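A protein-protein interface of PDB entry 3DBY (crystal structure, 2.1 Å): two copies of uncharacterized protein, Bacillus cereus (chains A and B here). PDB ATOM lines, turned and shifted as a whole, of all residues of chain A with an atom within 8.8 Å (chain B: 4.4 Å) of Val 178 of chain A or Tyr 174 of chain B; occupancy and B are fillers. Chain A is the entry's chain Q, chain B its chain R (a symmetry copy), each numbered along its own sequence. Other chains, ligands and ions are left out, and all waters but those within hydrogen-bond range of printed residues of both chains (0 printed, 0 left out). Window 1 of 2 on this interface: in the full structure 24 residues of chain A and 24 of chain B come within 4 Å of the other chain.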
ATOM      1  N   LEU A 131      -3.461  24.259  16.294  1.00  0.00           N
ATOM      2  CA  LEU A 131      -2.655  23.072  15.937  1.00  0.00           C
ATOM      3  C   LEU A 131      -1.793  22.547  17.096  1.00  0.00           C
ATOM      4  O   LEU A 131      -1.493  21.338  17.130  1.00  0.00           O
ATOM      5  CB  LEU A 131      -1.779  23.268  14.682  1.00  0.00           C
ATOM      6  CG  LEU A 131      -2.484  23.139  13.307  1.00  0.00           C
ATOM      7  CD1 LEU A 131      -1.577  23.525  12.153  1.00  0.00           C
ATOM      8  CD2 LEU A 131      -3.083  21.743  13.034  1.00  0.00           C
ATOM      9  N   HIS A 134      -4.224  20.241  18.903  1.00  0.00           N
ATOM     10  CA  HIS A 134      -4.403  19.050  18.091  1.00  0.00           C
ATOM     11  C   HIS A 134      -3.252  18.051  18.206  1.00  0.00           C
ATOM     12  O   HIS A 134      -3.456  16.829  18.269  1.00  0.00           O
ATOM     13  CB  HIS A 134      -4.493  19.482  16.625  1.00  0.00           C
ATOM     14  CG  HIS A 134      -5.784  20.163  16.278  1.00  0.00           C
ATOM     15  ND1 HIS A 134      -7.005  19.697  16.719  1.00  0.00           N
ATOM     16  CD2 HIS A 134      -6.048  21.218  15.469  1.00  0.00           C
ATOM     17  CE1 HIS A 134      -7.970  20.443  16.212  1.00  0.00           C
ATOM     18  NE2 HIS A 134      -7.415  21.374  15.451  1.00  0.00           N
ATOM     19  N   LEU A 135      -2.028  18.571  18.183  1.00  0.00           N
ATOM     20  CA  LEU A 135      -0.884  17.701  18.125  1.00  0.00           C
ATOM     21  C   LEU A 135      -0.684  17.045  19.472  1.00  0.00           C
ATOM     22  O   LEU A 135       0.060  16.014  19.568  1.00  0.00           O
ATOM     23  CB  LEU A 135       0.367  18.466  17.731  1.00  0.00           C
ATOM     24  CG  LEU A 135       0.505  18.887  16.269  1.00  0.00           C
ATOM     25  CD1 LEU A 135       1.744  19.713  16.197  1.00  0.00           C
ATOM     26  CD2 LEU A 135       0.589  17.665  15.353  1.00  0.00           C
ATOM     27  N   VAL A 136      -1.330  17.621  20.494  1.00  0.00           N
ATOM     28  CA  VAL A 136      -1.301  17.061  21.856  1.00  0.00           C
ATOM     29  C   VAL A 136      -2.483  16.129  22.143  1.00  0.00           C
ATOM     30  O   VAL A 136      -2.330  14.998  22.697  1.00  0.00           O
ATOM     31  CB  VAL A 136      -1.307  18.171  22.946  1.00  0.00           C
ATOM     32  CG1 VAL A 136      -1.448  17.521  24.329  1.00  0.00           C
ATOM     33  CG2 VAL A 136      -0.029  18.984  22.864  1.00  0.00           C
ATOM     34  N   LEU A 138      -5.034  14.837  20.102  1.00  0.00           N
ATOM     35  CA  LEU A 138      -5.561  13.885  19.161  1.00  0.00           C
ATOM     36  C   LEU A 138      -4.987  12.486  19.444  1.00  0.00           C
ATOM     37  O   LEU A 138      -5.717  11.532  19.527  1.00  0.00           O
ATOM     38  CB  LEU A 138      -5.223  14.336  17.736  1.00  0.00           C
ATOM     39  CG  LEU A 138      -6.175  15.438  17.247  1.00  0.00           C
ATOM     40  CD1 LEU A 138      -5.712  15.987  15.890  1.00  0.00           C
ATOM     41  CD2 LEU A 138      -7.667  14.948  17.215  1.00  0.00           C
ATOM     42  N   THR A 139      -3.668  12.357  19.592  1.00  0.00           N
ATOM     43  CA  THR A 139      -3.154  11.049  20.038  1.00  0.00           C
ATOM     44  C   THR A 139      -3.740  10.665  21.405  1.00  0.00           C
ATOM     45  O   THR A 139      -4.049   9.502  21.649  1.00  0.00           O
ATOM     46  CB  THR A 139      -1.630  11.013  20.138  1.00  0.00           C
ATOM     47  OG1 THR A 139      -1.231  12.117  20.943  1.00  0.00           O
ATOM     48  CG2 THR A 139      -0.981  11.099  18.708  1.00  0.00           C
ATOM     49  N   GLU A 171      -6.919   8.972  15.142  1.00  0.00           N
ATOM     50  CA  GLU A 171      -5.596   8.733  14.508  1.00  0.00           C
ATOM     51  C   GLU A 171      -5.530   9.416  13.122  1.00  0.00           C
ATOM     52  O   GLU A 171      -4.519  10.028  12.770  1.00  0.00           O
ATOM     53  CB  GLU A 171      -5.291   7.219  14.402  1.00  0.00           C
ATOM     54  CG  GLU A 171      -5.214   6.521  15.776  1.00  0.00           C
ATOM     55  CD  GLU A 171      -5.011   5.021  15.640  1.00  0.00           C
ATOM     56  OE1 GLU A 171      -5.478   4.443  14.643  1.00  0.00           O
ATOM     57  OE2 GLU A 171      -4.400   4.414  16.541  1.00  0.00           O
ATOM     58  N   GLN A 172      -6.631   9.341  12.367  1.00  0.00           N
ATOM     59  CA  GLN A 172      -6.704   9.959  11.037  1.00  0.00           C
ATOM     60  C   GLN A 172      -6.677  11.475  11.179  1.00  0.00           C
ATOM     61  O   GLN A 172      -5.984  12.151  10.413  1.00  0.00           O
ATOM     62  CB  GLN A 172      -8.022   9.584  10.349  1.00  0.00           C
ATOM     63  CG  GLN A 172      -8.248   8.100  10.068  1.00  0.00           C
ATOM     64  CD  GLN A 172      -9.620   7.874   9.368  1.00  0.00           C
ATOM     65  OE1 GLN A 172     -10.633   8.615   9.589  1.00  0.00           O
ATOM     66  NE2 GLN A 172      -9.658   6.878   8.526  1.00  0.00           N
ATOM     67  N   PHE A 173      -7.468  12.018  12.129  1.00  0.00           N
ATOM     68  CA  PHE A 173      -7.348  13.475  12.410  1.00  0.00           C
ATOM     69  C   PHE A 173      -5.878  13.844  12.759  1.00  0.00           C
ATOM     70  O   PHE A 173      -5.339  14.847  12.312  1.00  0.00           O
ATOM     71  CB  PHE A 173      -8.264  13.941  13.543  1.00  0.00           C
ATOM     72  CG  PHE A 173      -9.759  13.982  13.205  1.00  0.00           C
ATOM     73  CD1 PHE A 173     -10.230  14.561  12.038  1.00  0.00           C
ATOM     74  CD2 PHE A 173     -10.687  13.524  14.130  1.00  0.00           C
ATOM     75  CE1 PHE A 173     -11.612  14.629  11.776  1.00  0.00           C
ATOM     76  CE2 PHE A 173     -12.070  13.570  13.860  1.00  0.00           C
ATOM     77  CZ  PHE A 173     -12.522  14.135  12.711  1.00  0.00           C
ATOM     78  N   TYR A 174      -5.216  13.012  13.551  1.00  0.00           N
ATOM     79  CA  TYR A 174      -3.819  13.287  13.867  1.00  0.00           C
ATOM     80  C   TYR A 174      -2.906  13.373  12.643  1.00  0.00           C
ATOM     81  O   TYR A 174      -2.060  14.235  12.587  1.00  0.00           O
ATOM     82  CB  TYR A 174      -3.261  12.257  14.877  1.00  0.00           C
ATOM     83  CG  TYR A 174      -1.853  12.583  15.328  1.00  0.00           C
ATOM     84  CD1 TYR A 174      -1.598  13.667  16.197  1.00  0.00           C
ATOM     85  CD2 TYR A 174      -0.760  11.846  14.837  1.00  0.00           C
ATOM     86  CE1 TYR A 174      -0.270  13.978  16.612  1.00  0.00           C
ATOM     87  CE2 TYR A 174       0.536  12.138  15.226  1.00  0.00           C
ATOM     88  CZ  TYR A 174       0.774  13.215  16.117  1.00  0.00           C
ATOM     89  OH  TYR A 174       2.055  13.477  16.466  1.00  0.00           O
ATOM     90  N   LEU A 175      -3.030  12.436  11.700  1.00  0.00           N
ATOM     91  CA  LEU A 175      -2.204  12.439  10.500  1.00  0.00           C
ATOM     92  C   LEU A 175      -2.399  13.753   9.726  1.00  0.00           C
ATOM     93  O   LEU A 175      -1.442  14.351   9.214  1.00  0.00           O
ATOM     94  CB  LEU A 175      -2.551  11.205   9.638  1.00  0.00           C
ATOM     95  CG  LEU A 175      -2.203   9.863  10.291  1.00  0.00           C
ATOM     96  CD1 LEU A 175      -2.709   8.675   9.503  1.00  0.00           C
ATOM     97  CD2 LEU A 175      -0.749   9.742  10.508  1.00  0.00           C
ATOM     98  N   LYS A 176      -3.640  14.218   9.690  1.00  0.00           N
ATOM     99  CA  LYS A 176      -4.005  15.498   9.066  1.00  0.00           C
ATOM    100  C   LYS A 176      -3.432  16.744   9.777  1.00  0.00           C
ATOM    101  O   LYS A 176      -2.911  17.650   9.109  1.00  0.00           O
ATOM    102  CB  LYS A 176      -5.539  15.570   8.956  1.00  0.00           C
ATOM    103  CG  LYS A 176      -6.038  16.741   8.178  1.00  0.00           C
ATOM    104  CD  LYS A 176      -7.536  16.589   7.907  1.00  0.00           C
ATOM    105  CE  LYS A 176      -7.999  17.696   6.980  1.00  0.00           C
ATOM    106  NZ  LYS A 176      -9.448  17.598   6.661  1.00  0.00           N
ATOM    107  N   ALA A 177      -3.535  16.789  11.108  1.00  0.00           N
ATOM    108  CA  ALA A 177      -2.855  17.805  11.946  1.00  0.00           C
ATOM    109  C   ALA A 177      -1.335  17.874  11.669  1.00  0.00           C
ATOM    110  O   ALA A 177      -0.743  18.961  11.607  1.00  0.00           O
ATOM    111  CB  ALA A 177      -3.121  17.546  13.504  1.00  0.00           C
ATOM    112  N   VAL A 178      -0.699  16.705  11.536  1.00  0.00           N
ATOM    113  CA  VAL A 178       0.720  16.633  11.293  1.00  0.00           C
ATOM    114  C   VAL A 178       1.067  17.287   9.956  1.00  0.00           C
ATOM    115  O   VAL A 178       2.028  18.072   9.869  1.00  0.00           O
ATOM    116  CB  VAL A 178       1.232  15.140  11.316  1.00  0.00           C
ATOM    117  CG1 VAL A 178       2.593  15.055  10.651  1.00  0.00           C
ATOM    118  CG2 VAL A 178       1.264  14.616  12.775  1.00  0.00           C
ATOM    119  N   GLU A 179       0.314  16.961   8.905  1.00  0.00           N
ATOM    120  CA  GLU A 179       0.547  17.570   7.597  1.00  0.00           C
ATOM    121  C   GLU A 179       0.283  19.091   7.602  1.00  0.00           C
ATOM    122  O   GLU A 179       1.073  19.870   7.054  1.00  0.00           O
ATOM    123  CB  GLU A 179      -0.253  16.856   6.483  1.00  0.00           C
ATOM    124  CG  GLU A 179       0.105  15.357   6.335  1.00  0.00           C
ATOM    125  CD  GLU A 179       1.585  15.070   5.905  1.00  0.00           C
ATOM    126  OE1 GLU A 179       2.034  13.897   6.020  1.00  0.00           O
ATOM    127  OE2 GLU A 179       2.303  16.003   5.432  1.00  0.00           O
ATOM    128  N   MET A 180      -0.793  19.529   8.239  1.00  0.00           N
ATOM    129  CA  MET A 180      -1.148  20.962   8.214  1.00  0.00           C
ATOM    130  C   MET A 180      -0.132  21.754   9.002  1.00  0.00           C
ATOM    131  O   MET A 180       0.037  22.952   8.786  1.00  0.00           O
ATOM    132  CB  MET A 180      -2.532  21.218   8.824  1.00  0.00           C
ATOM    133  CG  MET A 180      -3.652  20.424   8.167  1.00  0.00           C
ATOM    134  SD  MET A 180      -5.292  21.077   8.419  1.00  0.00           S
ATOM    135  CE  MET A 180      -5.116  22.058   7.020  1.00  0.00           C
ATOM    136  N   THR A 181       0.506  21.091   9.956  1.00  0.00           N
ATOM    137  CA  THR A 181       1.509  21.761  10.735  1.00  0.00           C
ATOM    138  C   THR A 181       2.668  22.125   9.817  1.00  0.00           C
ATOM    139  O   THR A 181       3.283  23.189   9.977  1.00  0.00           O
ATOM    140  CB  THR A 181       1.960  20.934  11.951  1.00  0.00           C
ATOM    141  OG1 THR A 181       0.867  20.848  12.904  1.00  0.00           O
ATOM    142  CG2 THR A 181       3.166  21.646  12.620  1.00  0.00           C
ATOM    143  N   GLY A 182       2.915  21.267   8.812  1.00  0.00           N
ATOM    144  CA  GLY A 182       3.954  21.484   7.823  1.00  0.00           C
ATOM    145  C   GLY A 182       3.569  22.568   6.812  1.00  0.00           C
ATOM    146  O   GLY A 182       4.444  23.285   6.272  1.00  0.00           O
ATOM    147  N   TYR A 183       2.267  22.667   6.526  1.00  0.00           N
ATOM    148  CA  TYR A 183       1.734  23.747   5.696  1.00  0.00           C
ATOM    149  C   TYR A 183       2.074  25.113   6.338  1.00  0.00           C
ATOM    150  O   TYR A 183       2.268  26.088   5.625  1.00  0.00           O
ATOM    151  CB  TYR A 183       0.212  23.661   5.527  1.00  0.00           C
ATOM    152  CG  TYR A 183      -0.359  22.366   4.895  1.00  0.00           C
ATOM    153  CD1 TYR A 183       0.464  21.360   4.387  1.00  0.00           C
ATOM    154  CD2 TYR A 183      -1.720  22.171   4.834  1.00  0.00           C
ATOM    155  CE1 TYR A 183      -0.080  20.178   3.826  1.00  0.00           C
ATOM    156  CE2 TYR A 183      -2.281  21.013   4.256  1.00  0.00           C
ATOM    157  CZ  TYR A 183      -1.465  20.010   3.769  1.00  0.00           C
ATOM    158  OH  TYR A 183      -2.053  18.850   3.222  1.00  0.00           O
ATOM    159  N   LEU A 184       2.163  25.163   7.673  1.00  0.00           N
ATOM    160  CA  LEU A 184       2.513  26.407   8.371  1.00  0.00           C
ATOM    161  C   LEU A 184       3.856  26.955   7.922  1.00  0.00           C
ATOM    162  O   LEU A 184       4.177  28.099   8.208  1.00  0.00           O
ATOM    163  CB  LEU A 184       2.556  26.210   9.902  1.00  0.00           C
ATOM    164  CG  LEU A 184       1.264  25.829  10.665  1.00  0.00           C
ATOM    165  CD1 LEU A 184       1.481  25.760  12.212  1.00  0.00           C
ATOM    166  CD2 LEU A 184       0.138  26.731  10.350  1.00  0.00           C
ATOM    167  N   ARG A 185       4.685  26.122   7.299  1.00  0.00           N
ATOM    168  CA  ARG A 185       5.987  26.577   6.807  1.00  0.00           C
ATOM    169  C   ARG A 185       5.780  27.619   5.721  1.00  0.00           C
ATOM    170  O   ARG A 185       6.701  28.349   5.369  1.00  0.00           O
ATOM    171  CB  ARG A 185       6.856  25.401   6.291  1.00  0.00           C
ATOM    172  CG  ARG A 185       7.575  24.650   7.425  1.00  0.00           C
ATOM    173  CD  ARG A 185       8.184  23.340   6.978  1.00  0.00           C
ATOM    174  NE  ARG A 185       7.198  22.431   6.372  1.00  0.00           N
ATOM    175  CZ  ARG A 185       7.493  21.185   6.004  1.00  0.00           C
ATOM    176  NH1 ARG A 185       8.716  20.741   6.203  1.00  0.00           N
ATOM    177  NH2 ARG A 185       6.588  20.385   5.450  1.00  0.00           N
ATOM    178  N   PHE A 197     -11.000  21.844   9.564  1.00  0.00           N
ATOM    179  CA  PHE A 197     -10.468  20.735  10.363  1.00  0.00           C
ATOM    180  C   PHE A 197     -10.869  20.839  11.837  1.00  0.00           C
ATOM    181  O   PHE A 197     -11.340  19.885  12.447  1.00  0.00           O
ATOM    182  CB  PHE A 197      -8.927  20.744  10.232  1.00  0.00           C
ATOM    183  CG  PHE A 197      -8.234  19.675  11.026  1.00  0.00           C
ATOM    184  CD1 PHE A 197      -8.552  18.333  10.856  1.00  0.00           C
ATOM    185  CD2 PHE A 197      -7.262  20.007  11.949  1.00  0.00           C
ATOM    186  CE1 PHE A 197      -7.898  17.324  11.579  1.00  0.00           C
ATOM    187  CE2 PHE A 197      -6.604  19.000  12.646  1.00  0.00           C
ATOM    188  CZ  PHE A 197      -6.949  17.664  12.470  1.00  0.00           C
ATOM    189  N   LEU B 135      10.559   9.295  11.547  1.00  0.00           N
ATOM    190  CA  LEU B 135       9.689  10.501  11.594  1.00  0.00           C
ATOM    191  C   LEU B 135       9.612  11.295  10.275  1.00  0.00           C
ATOM    192  O   LEU B 135       8.650  12.000  10.021  1.00  0.00           O
ATOM    193  CB  LEU B 135      10.136  11.436  12.701  1.00  0.00           C
ATOM    194  CG  LEU B 135       9.845  10.820  14.068  1.00  0.00           C
ATOM    195  CD1 LEU B 135      10.556  11.608  15.120  1.00  0.00           C
ATOM    196  CD2 LEU B 135       8.274  10.707  14.298  1.00  0.00           C
ATOM    197  N   LEU B 138       8.468   7.817   7.056  1.00  0.00           N
ATOM    198  CA  LEU B 138       7.294   6.970   7.166  1.00  0.00           C
ATOM    199  C   LEU B 138       6.059   7.674   6.577  1.00  0.00           C
ATOM    200  O   LEU B 138       5.300   7.084   5.767  1.00  0.00           O
ATOM    201  CB  LEU B 138       7.052   6.535   8.606  1.00  0.00           C
ATOM    202  CG  LEU B 138       7.886   5.379   9.156  1.00  0.00           C
ATOM    203  CD1 LEU B 138       7.676   5.270  10.692  1.00  0.00           C
ATOM    204  CD2 LEU B 138       7.605   4.025   8.413  1.00  0.00           C
ATOM    205  N   THR B 139       5.852   8.945   6.935  1.00  0.00           N
ATOM    206  CA  THR B 139       4.764   9.695   6.254  1.00  0.00           C
ATOM    207  C   THR B 139       5.076   9.787   4.757  1.00  0.00           C
ATOM    208  O   THR B 139       4.204   9.664   3.920  1.00  0.00           O
ATOM    209  CB  THR B 139       4.529  11.138   6.828  1.00  0.00           C
ATOM    210  OG1 THR B 139       5.660  11.944   6.559  1.00  0.00           O
ATOM    211  CG2 THR B 139       4.288  11.139   8.309  1.00  0.00           C
ATOM    212  N   PHE B 170       2.292   1.988   6.590  1.00  0.00           N
ATOM    213  CA  PHE B 170       3.249   3.046   6.864  1.00  0.00           C
ATOM    214  C   PHE B 170       2.717   4.104   7.818  1.00  0.00           C
ATOM    215  O   PHE B 170       3.463   4.641   8.674  1.00  0.00           O
ATOM    216  CB  PHE B 170       3.741   3.676   5.527  1.00  0.00           C
ATOM    217  CG  PHE B 170       4.669   2.763   4.752  1.00  0.00           C
ATOM    218  CD1 PHE B 170       5.799   2.242   5.372  1.00  0.00           C
ATOM    219  CD2 PHE B 170       4.423   2.427   3.424  1.00  0.00           C
ATOM    220  CE1 PHE B 170       6.671   1.388   4.702  1.00  0.00           C
ATOM    221  CE2 PHE B 170       5.312   1.603   2.723  1.00  0.00           C
ATOM    222  CZ  PHE B 170       6.425   1.081   3.366  1.00  0.00           C
ATOM    223  N   GLU B 171       1.425   4.422   7.657  1.00  0.00           N
ATOM    224  CA  GLU B 171       0.738   5.255   8.620  1.00  0.00           C
ATOM    225  C   GLU B 171       0.764   4.636  10.028  1.00  0.00           C
ATOM    226  O   GLU B 171       1.008   5.339  11.002  1.00  0.00           O
ATOM    227  CB  GLU B 171      -0.704   5.564   8.147  1.00  0.00           C
ATOM    228  CG  GLU B 171      -0.762   6.495   6.905  1.00  0.00           C
ATOM    229  CD  GLU B 171      -2.192   6.698   6.410  1.00  0.00           C
ATOM    230  OE1 GLU B 171      -3.056   5.866   6.725  1.00  0.00           O
ATOM    231  OE2 GLU B 171      -2.451   7.679   5.694  1.00  0.00           O
ATOM    232  N   GLN B 172       0.495   3.335  10.143  1.00  0.00           N
ATOM    233  CA  GLN B 172       0.515   2.719  11.454  1.00  0.00           C
ATOM    234  C   GLN B 172       1.930   2.752  12.037  1.00  0.00           C
ATOM    235  O   GLN B 172       2.100   2.942  13.248  1.00  0.00           O
ATOM    236  CB  GLN B 172       0.064   1.271  11.374  1.00  0.00           C
ATOM    237  CG  GLN B 172      -1.387   1.064  10.923  1.00  0.00           C
ATOM    238  CD  GLN B 172      -1.704  -0.421  10.651  1.00  0.00           C
ATOM    239  OE1 GLN B 172      -0.843  -1.250  10.206  1.00  0.00           O
ATOM    240  NE2 GLN B 172      -2.936  -0.762  10.909  1.00  0.00           N
ATOM    241  N   PHE B 173       2.942   2.531  11.182  1.00  0.00           N
ATOM    242  CA  PHE B 173       4.327   2.595  11.647  1.00  0.00           C
ATOM    243  C   PHE B 173       4.666   4.026  12.136  1.00  0.00           C
ATOM    244  O   PHE B 173       5.335   4.229  13.162  1.00  0.00           O
ATOM    245  CB  PHE B 173       5.311   2.185  10.516  1.00  0.00           C
ATOM    246  CG  PHE B 173       5.423   0.693  10.272  1.00  0.00           C
ATOM    247  CD1 PHE B 173       5.433  -0.222  11.338  1.00  0.00           C
ATOM    248  CD2 PHE B 173       5.603   0.222   8.979  1.00  0.00           C
ATOM    249  CE1 PHE B 173       5.630  -1.610  11.112  1.00  0.00           C
ATOM    250  CE2 PHE B 173       5.762  -1.179   8.718  1.00  0.00           C
ATOM    251  CZ  PHE B 173       5.776  -2.086   9.793  1.00  0.00           C
ATOM    252  N   TYR B 174       4.186   5.006  11.400  1.00  0.00           N
ATOM    253  CA  TYR B 174       4.355   6.408  11.794  1.00  0.00           C
ATOM    254  C   TYR B 174       3.810   6.641  13.216  1.00  0.00           C
ATOM    255  O   TYR B 174       4.513   7.175  14.065  1.00  0.00           O
ATOM    256  CB  TYR B 174       3.763   7.400  10.752  1.00  0.00           C
ATOM    257  CG  TYR B 174       4.000   8.836  11.168  1.00  0.00           C
ATOM    258  CD1 TYR B 174       5.299   9.389  11.124  1.00  0.00           C
ATOM    259  CD2 TYR B 174       2.952   9.624  11.686  1.00  0.00           C
ATOM    260  CE1 TYR B 174       5.540  10.693  11.555  1.00  0.00           C
ATOM    261  CE2 TYR B 174       3.169  10.939  12.099  1.00  0.00           C
ATOM    262  CZ  TYR B 174       4.468  11.462  12.028  1.00  0.00           C
ATOM    263  OH  TYR B 174       4.721  12.733  12.435  1.00  0.00           O
ATOM    264  N   LEU B 175       2.590   6.201  13.508  1.00  0.00           N
ATOM    265  CA  LEU B 175       2.035   6.439  14.846  1.00  0.00           C
ATOM    266  C   LEU B 175       2.906   5.795  15.946  1.00  0.00           C
ATOM    267  O   LEU B 175       3.157   6.433  16.994  1.00  0.00           O
ATOM    268  CB  LEU B 175       0.591   5.950  14.938  1.00  0.00           C
ATOM    269  CG  LEU B 175      -0.344   6.607  13.913  1.00  0.00           C
ATOM    270  CD1 LEU B 175      -1.634   5.778  13.815  1.00  0.00           C
ATOM    271  CD2 LEU B 175      -0.632   8.046  14.312  1.00  0.00           C
ATOM    272  N   LYS B 176       3.374   4.558  15.687  1.00  0.00           N
ATOM    273  CA  LYS B 176       4.329   3.868  16.553  1.00  0.00           C
ATOM    274  C   LYS B 176       5.638   4.655  16.742  1.00  0.00           C
ATOM    275  O   LYS B 176       6.169   4.735  17.852  1.00  0.00           O
ATOM    276  CB  LYS B 176       4.639   2.458  16.003  1.00  0.00           C
ATOM    277  CG  LYS B 176       5.448   1.556  16.974  1.00  0.00           C
ATOM    278  CD  LYS B 176       5.150   0.042  16.711  1.00  0.00           C
ATOM    279  CE  LYS B 176       6.131  -0.852  17.487  1.00  0.00           C
ATOM    280  NZ  LYS B 176       5.974  -2.328  17.139  1.00  0.00           N
ATOM    281  N   ALA B 177       6.184   5.199  15.653  1.00  0.00           N
ATOM    282  CA  ALA B 177       7.403   6.005  15.774  1.00  0.00           C
ATOM    283  C   ALA B 177       7.156   7.252  16.622  1.00  0.00           C
ATOM    284  O   ALA B 177       7.970   7.600  17.442  1.00  0.00           O
ATOM    285  CB  ALA B 177       7.960   6.392  14.394  1.00  0.00           C
ATOM    286  N   VAL B 178       6.009   7.895  16.450  1.00  0.00           N
ATOM    287  CA  VAL B 178       5.651   9.077  17.278  1.00  0.00           C
ATOM    288  C   VAL B 178       5.682   8.716  18.773  1.00  0.00           C
ATOM    289  O   VAL B 178       6.200   9.475  19.589  1.00  0.00           O
ATOM    290  CB  VAL B 178       4.246   9.684  16.868  1.00  0.00           C
ATOM    291  CG1 VAL B 178       3.704  10.597  17.950  1.00  0.00           C
ATOM    292  CG2 VAL B 178       4.351  10.439  15.534  1.00  0.00           C
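Val 178 of chain A touches one residue of chain B.
Printed residues of chain A within 4 Å of Glu 171 of chain B: Leu 175 (3.7 Å).
Of the printed residues of chain A, Val 178 of chain B touches Tyr 174.
Of the printed residues of chain B, Tyr 174 of chain A touches Leu 175 and Val 178.
Gly 182 of chain A touches none of the printed residues of chain B.
The nearest printed residue of chain B that does not touch Tyr 174 of chain A is Tyr 174 of chain B (4.3 Å).
Among the printed residues, pairs that only touch across the chains: Val 178 of chain A with Tyr 174 of chain B, Tyr 174 of chain A with Val 178 of chain B, Leu 175 of chain A with Glu 171 of chain B, Glu 179 of chain A with Thr 139 of chain B, Tyr 174 of chain A with Leu 175 of chain B, Leu 175 of chain A with Tyr 174 of chain B and Glu 171 of chain A with Leu 175 of chain B.
Hydrophobic or aromatic side chains of chain A within 4 Å of the printed part of chain B: Tyr 174, Leu 175 and Val 178.
Of the 12 printed residues of chain B, 5 touch a printed residue of chain A.
Among the printed residues, no Asp or Glu carboxylate lies within 4 Å of a Lys or Arg side-chain nitrogen of the other chain.
Glu 171 of chain A touches Leu 175 of chain B, and with the chains exchanged Leu 175 of chain A touches Glu 171 of chain B.
Tyr 174 of chain A touches Leu 175 of chain B, and with the chains exchanged Leu 175 of chain A touches Tyr 174 of chain B.
Tyr 174 of chain A touches Val 178 of chain B, and with the chains exchanged Val 178 of chain A touches Tyr 174 of chain B.
Positions printed for both chains: 135, 138, 139, 171, 172, 173, 174, 175, 176, 177 and 178.
Of the 7 pairs that touch across the chains among the printed residues, 6 have their exchanged pair printed and touching as well.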
